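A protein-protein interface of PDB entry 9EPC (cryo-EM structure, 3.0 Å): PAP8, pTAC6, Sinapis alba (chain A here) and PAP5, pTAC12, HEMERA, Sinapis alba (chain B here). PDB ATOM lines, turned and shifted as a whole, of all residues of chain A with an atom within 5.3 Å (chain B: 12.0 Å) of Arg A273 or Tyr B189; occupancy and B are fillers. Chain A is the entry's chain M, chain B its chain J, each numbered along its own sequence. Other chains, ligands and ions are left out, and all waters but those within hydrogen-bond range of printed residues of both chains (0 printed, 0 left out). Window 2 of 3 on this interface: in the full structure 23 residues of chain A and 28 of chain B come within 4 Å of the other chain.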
ATOM      1  N   TYR A 233     -23.062  -7.079 -13.972  1.00  0.00           N
ATOM      2  CA  TYR A 233     -23.880  -6.340 -13.019  1.00  0.00           C
ATOM      3  C   TYR A 233     -25.202  -5.953 -13.670  1.00  0.00           C
ATOM      4  O   TYR A 233     -25.217  -5.307 -14.722  1.00  0.00           O
ATOM      5  CB  TYR A 233     -23.135  -5.105 -12.527  1.00  0.00           C
ATOM      6  CG  TYR A 233     -23.825  -4.387 -11.394  1.00  0.00           C
ATOM      7  CD1 TYR A 233     -23.875  -4.942 -10.124  1.00  0.00           C
ATOM      8  CD2 TYR A 233     -24.419  -3.149 -11.590  1.00  0.00           C
ATOM      9  CE1 TYR A 233     -24.503  -4.290  -9.084  1.00  0.00           C
ATOM     10  CE2 TYR A 233     -25.049  -2.488 -10.555  1.00  0.00           C
ATOM     11  CZ  TYR A 233     -25.087  -3.063  -9.304  1.00  0.00           C
ATOM     12  OH  TYR A 233     -25.714  -2.409  -8.270  1.00  0.00           O
ATOM     13  N   GLU A 248     -19.424 -10.099  -7.045  1.00  0.00           N
ATOM     14  CA  GLU A 248     -20.049 -10.854  -5.964  1.00  0.00           C
ATOM     15  C   GLU A 248     -20.442 -12.251  -6.423  1.00  0.00           C
ATOM     16  O   GLU A 248     -20.272 -13.227  -5.685  1.00  0.00           O
ATOM     17  CB  GLU A 248     -21.270 -10.104  -5.431  1.00  0.00           C
ATOM     18  CG  GLU A 248     -20.977  -9.154  -4.281  1.00  0.00           C
ATOM     19  CD  GLU A 248     -20.273  -7.889  -4.721  1.00  0.00           C
ATOM     20  OE1 GLU A 248     -20.136  -7.674  -5.944  1.00  0.00           O
ATOM     21  OE2 GLU A 248     -19.860  -7.104  -3.844  1.00  0.00           O
ATOM     22  N   LEU A 266     -14.483 -12.495  -0.688  1.00  0.00           N
ATOM     23  CA  LEU A 266     -14.376 -11.571   0.432  1.00  0.00           C
ATOM     24  C   LEU A 266     -14.265 -10.153  -0.113  1.00  0.00           C
ATOM     25  O   LEU A 266     -13.332  -9.845  -0.859  1.00  0.00           O
ATOM     26  CB  LEU A 266     -13.167 -11.908   1.301  1.00  0.00           C
ATOM     27  CG  LEU A 266     -12.737 -10.840   2.306  1.00  0.00           C
ATOM     28  CD1 LEU A 266     -13.823 -10.605   3.335  1.00  0.00           C
ATOM     29  CD2 LEU A 266     -11.436 -11.235   2.978  1.00  0.00           C
ATOM     30  N   VAL A 267     -15.207  -9.298   0.262  1.00  0.00           N
ATOM     31  CA  VAL A 267     -15.255  -7.924  -0.222  1.00  0.00           C
ATOM     32  C   VAL A 267     -14.619  -7.023   0.826  1.00  0.00           C
ATOM     33  O   VAL A 267     -15.132  -6.899   1.944  1.00  0.00           O
ATOM     34  CB  VAL A 267     -16.695  -7.485  -0.525  1.00  0.00           C
ATOM     35  CG1 VAL A 267     -16.717  -6.044  -0.999  1.00  0.00           C
ATOM     36  CG2 VAL A 267     -17.315  -8.401  -1.560  1.00  0.00           C
ATOM     37  N   GLY A 271     -17.797   0.566   1.386  1.00  0.00           N
ATOM     38  CA  GLY A 271     -18.989   1.026   0.705  1.00  0.00           C
ATOM     39  C   GLY A 271     -20.119   0.020   0.733  1.00  0.00           C
ATOM     40  O   GLY A 271     -21.271   0.361   0.447  1.00  0.00           O
ATOM     41  N   GLY A 272     -19.799  -1.228   1.073  1.00  0.00           N
ATOM     42  CA  GLY A 272     -20.823  -2.251   1.157  1.00  0.00           C
ATOM     43  C   GLY A 272     -21.431  -2.562  -0.200  1.00  0.00           C
ATOM     44  O   GLY A 272     -20.796  -2.424  -1.249  1.00  0.00           O
ATOM     45  N   ARG A 273     -22.695  -2.987  -0.172  1.00  0.00           N
ATOM     46  CA  ARG A 273     -23.394  -3.323  -1.406  1.00  0.00           C
ATOM     47  C   ARG A 273     -23.724  -2.091  -2.238  1.00  0.00           C
ATOM     48  O   ARG A 273     -24.055  -2.227  -3.420  1.00  0.00           O
ATOM     49  CB  ARG A 273     -24.675  -4.096  -1.093  1.00  0.00           C
ATOM     50  CG  ARG A 273     -24.529  -5.121   0.021  1.00  0.00           C
ATOM     51  CD  ARG A 273     -25.099  -4.597   1.330  1.00  0.00           C
ATOM     52  NE  ARG A 273     -24.781  -5.468   2.456  1.00  0.00           N
ATOM     53  CZ  ARG A 273     -23.773  -5.269   3.294  1.00  0.00           C
ATOM     54  NH1 ARG A 273     -22.964  -4.230   3.168  1.00  0.00           N
ATOM     55  NH2 ARG A 273     -23.574  -6.133   4.286  1.00  0.00           N
ATOM     56  N   LYS A 274     -23.642  -0.900  -1.651  1.00  0.00           N
ATOM     57  CA  LYS A 274     -23.949   0.342  -2.343  1.00  0.00           C
ATOM     58  C   LYS A 274     -22.720   0.986  -2.969  1.00  0.00           C
ATOM     59  O   LYS A 274     -22.819   2.098  -3.498  1.00  0.00           O
ATOM     60  CB  LYS A 274     -24.614   1.329  -1.380  1.00  0.00           C
ATOM     61  CG  LYS A 274     -25.718   0.724  -0.529  1.00  0.00           C
ATOM     62  CD  LYS A 274     -26.838   0.158  -1.385  1.00  0.00           C
ATOM     63  CE  LYS A 274     -27.938  -0.439  -0.522  1.00  0.00           C
ATOM     64  NZ  LYS A 274     -29.031  -1.033  -1.339  1.00  0.00           N
ATOM     65  N   ARG A 275     -21.572   0.316  -2.920  1.00  0.00           N
ATOM     66  CA  ARG A 275     -20.331   0.888  -3.418  1.00  0.00           C
ATOM     67  C   ARG A 275     -20.390   1.076  -4.933  1.00  0.00           C
ATOM     68  O   ARG A 275     -21.317   0.629  -5.613  1.00  0.00           O
ATOM     69  CB  ARG A 275     -19.149  -0.007  -3.054  1.00  0.00           C
ATOM     70  CG  ARG A 275     -19.074  -1.263  -3.897  1.00  0.00           C
ATOM     71  CD  ARG A 275     -17.949  -2.174  -3.452  1.00  0.00           C
ATOM     72  NE  ARG A 275     -17.763  -3.278  -4.384  1.00  0.00           N
ATOM     73  CZ  ARG A 275     -18.479  -4.393  -4.375  1.00  0.00           C
ATOM     74  NH1 ARG A 275     -19.438  -4.591  -3.486  1.00  0.00           N
ATOM     75  NH2 ARG A 275     -18.228  -5.332  -5.282  1.00  0.00           N
ATOM     76  N   ARG A 277     -19.105   0.036  -8.377  1.00  0.00           N
ATOM     77  CA  ARG A 277     -18.501  -1.174  -8.922  1.00  0.00           C
ATOM     78  C   ARG A 277     -17.294  -0.886  -9.802  1.00  0.00           C
ATOM     79  O   ARG A 277     -16.480  -1.787 -10.026  1.00  0.00           O
ATOM     80  CB  ARG A 277     -19.542  -1.956  -9.720  1.00  0.00           C
ATOM     81  CG  ARG A 277     -20.822  -2.234  -8.961  1.00  0.00           C
ATOM     82  CD  ARG A 277     -20.655  -3.394  -8.005  1.00  0.00           C
ATOM     83  NE  ARG A 277     -21.880  -3.655  -7.260  1.00  0.00           N
ATOM     84  CZ  ARG A 277     -22.166  -4.810  -6.676  1.00  0.00           C
ATOM     85  NH1 ARG A 277     -21.346  -5.843  -6.752  1.00  0.00           N
ATOM     86  NH2 ARG A 277     -23.307  -4.932  -6.005  1.00  0.00           N
ATOM     87  N   ASN B 184     -27.576 -15.507  -0.799  1.00  0.00           N
ATOM     88  CA  ASN B 184     -26.152 -15.204  -0.745  1.00  0.00           C
ATOM     89  C   ASN B 184     -25.414 -16.185   0.156  1.00  0.00           C
ATOM     90  O   ASN B 184     -25.483 -17.398  -0.040  1.00  0.00           O
ATOM     91  CB  ASN B 184     -25.926 -13.773  -0.254  1.00  0.00           C
ATOM     92  CG  ASN B 184     -26.640 -12.746  -1.107  1.00  0.00           C
ATOM     93  OD1 ASN B 184     -26.900 -12.976  -2.288  1.00  0.00           O
ATOM     94  ND2 ASN B 184     -26.958 -11.602  -0.513  1.00  0.00           N
ATOM     95  N   GLY B 185     -24.709 -15.650   1.150  1.00  0.00           N
ATOM     96  CA  GLY B 185     -23.911 -16.453   2.049  1.00  0.00           C
ATOM     97  C   GLY B 185     -22.491 -16.699   1.592  1.00  0.00           C
ATOM     98  O   GLY B 185     -21.699 -17.263   2.358  1.00  0.00           O
ATOM     99  N   PHE B 186     -22.143 -16.298   0.369  1.00  0.00           N
ATOM    100  CA  PHE B 186     -20.793 -16.452  -0.149  1.00  0.00           C
ATOM    101  C   PHE B 186     -20.011 -15.149  -0.193  1.00  0.00           C
ATOM    102  O   PHE B 186     -18.837 -15.166  -0.576  1.00  0.00           O
ATOM    103  CB  PHE B 186     -20.831 -17.065  -1.555  1.00  0.00           C
ATOM    104  CG  PHE B 186     -21.274 -18.498  -1.580  1.00  0.00           C
ATOM    105  CD1 PHE B 186     -22.618 -18.822  -1.588  1.00  0.00           C
ATOM    106  CD2 PHE B 186     -20.345 -19.521  -1.597  1.00  0.00           C
ATOM    107  CE1 PHE B 186     -23.025 -20.139  -1.612  1.00  0.00           C
ATOM    108  CE2 PHE B 186     -20.746 -20.839  -1.620  1.00  0.00           C
ATOM    109  CZ  PHE B 186     -22.087 -21.149  -1.627  1.00  0.00           C
ATOM    110  N   VAL B 187     -20.621 -14.030   0.186  1.00  0.00           N
ATOM    111  CA  VAL B 187     -19.970 -12.728   0.175  1.00  0.00           C
ATOM    112  C   VAL B 187     -19.765 -12.275   1.614  1.00  0.00           C
ATOM    113  O   VAL B 187     -20.653 -12.425   2.459  1.00  0.00           O
ATOM    114  CB  VAL B 187     -20.784 -11.693  -0.627  1.00  0.00           C
ATOM    115  CG1 VAL B 187     -20.848 -12.095  -2.085  1.00  0.00           C
ATOM    116  CG2 VAL B 187     -22.188 -11.556  -0.065  1.00  0.00           C
ATOM    117  N   VAL B 188     -18.578 -11.746   1.895  1.00  0.00           N
ATOM    118  CA  VAL B 188     -18.229 -11.242   3.216  1.00  0.00           C
ATOM    119  C   VAL B 188     -17.717  -9.820   3.056  1.00  0.00           C
ATOM    120  O   VAL B 188     -16.836  -9.564   2.229  1.00  0.00           O
ATOM    121  CB  VAL B 188     -17.170 -12.122   3.905  1.00  0.00           C
ATOM    122  CG1 VAL B 188     -16.827 -11.563   5.273  1.00  0.00           C
ATOM    123  CG2 VAL B 188     -17.662 -13.554   4.019  1.00  0.00           C
ATOM    124  N   TYR B 189     -18.265  -8.901   3.843  1.00  0.00           N
ATOM    125  CA  TYR B 189     -17.880  -7.498   3.799  1.00  0.00           C
ATOM    126  C   TYR B 189     -17.071  -7.154   5.041  1.00  0.00           C
ATOM    127  O   TYR B 189     -17.496  -7.442   6.164  1.00  0.00           O
ATOM    128  CB  TYR B 189     -19.109  -6.594   3.707  1.00  0.00           C
ATOM    129  CG  TYR B 189     -19.912  -6.775   2.442  1.00  0.00           C
ATOM    130  CD1 TYR B 189     -20.885  -7.758   2.350  1.00  0.00           C
ATOM    131  CD2 TYR B 189     -19.702  -5.956   1.342  1.00  0.00           C
ATOM    132  CE1 TYR B 189     -21.623  -7.924   1.197  1.00  0.00           C
ATOM    133  CE2 TYR B 189     -20.437  -6.114   0.187  1.00  0.00           C
ATOM    134  CZ  TYR B 189     -21.395  -7.100   0.119  1.00  0.00           C
ATOM    135  OH  TYR B 189     -22.130  -7.262  -1.033  1.00  0.00           O
ATOM    136  N   ASN B 190     -15.908  -6.544   4.835  1.00  0.00           N
ATOM    137  CA  ASN B 190     -15.064  -6.107   5.940  1.00  0.00           C
ATOM    138  C   ASN B 190     -14.778  -4.613   5.847  1.00  0.00           C
ATOM    139  O   ASN B 190     -15.676  -3.815   5.579  1.00  0.00           O
ATOM    140  CB  ASN B 190     -13.751  -6.892   5.961  1.00  0.00           C
ATOM    141  CG  ASN B 190     -13.927  -8.308   6.469  1.00  0.00           C
ATOM    142  OD1 ASN B 190     -15.040  -8.830   6.519  1.00  0.00           O
ATOM    143  ND2 ASN B 190     -12.824  -8.939   6.853  1.00  0.00           N
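The backbone carbonyl oxygen (O) of Val B188 lies within hydrogen-bond range of the backbone NH (N) of Val A267, 2.6 Å away. O of Val A267 is in hydrogen-bond range of N of Asn B190, at 3.0 Å.
The guanidinium group of Arg A275 lies within salt-bridge range of the side-chain carboxylate of Glu A248. OE2 of Glu A248 lies within salt-bridge range of NH1 of Arg A277 (3.5 Å). O of Gly A272 sits close to NH1 of Arg A275 (3.4 Å).
Val B187 touches Glu A248. Glu A248 touches Tyr B189 (OE2 to OH, 3.6 Å). Leu A266 touches Val B188. Leu A266 touches Asn B190 (CD1 to OD1, 3.8 Å). CA of Tyr B189 touches O of Val A267, at 3.4 Å. C of Gly A272 touches CE2 of Tyr B189, at 3.7 Å. Tyr B189 touches Arg A273 (OH to CG, 3.4 Å).
Of chain B, only Val B187 and Tyr B189 come within 4 Å of Glu A248. Val A267 touches just these residues of chain B: Val B188 (2.6 Å), Tyr B189 (3.4 Å) and Asn B190 (3.0 Å). Gly A271 touches none of the printed residues of chain B. Gly A272 touches one residue of chain B. No residue of chain B comes within 4 Å of Lys A274. Arg A277 touches none of the printed residues of chain B. Gly B185 touches none of the printed residues of chain A. Printed residues of chain A within 4 Å of Val B187: Glu A248. Of chain A, only Glu A248, Val A267, Gly A272 and Arg A273 come within 4 Å of Tyr B189. Of the printed residues of chain A, Asn B190 touches Leu A266 and Val A267. The nearest residue of chain A that does not touch Tyr B189 is Arg A275 (4.1 Å). The nearest printed residue of chain A that does not touch Asn B190 is Gly A271 (6.4 Å).
Printed residues of chain A that touch a printed residue of chain B: Glu A248, Leu A266, Val A267, Gly A272 and Arg A273. Hydrophobic or aromatic side chains of chain A within 4 Å of the printed part of chain B: Leu A266 and Val A267. Among the printed residues, 9 pairs touch across the chains. Among the printed residues, no Asp or Glu carboxylate lies within 4 Å of a Lys or Arg side-chain nitrogen of the other chain.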
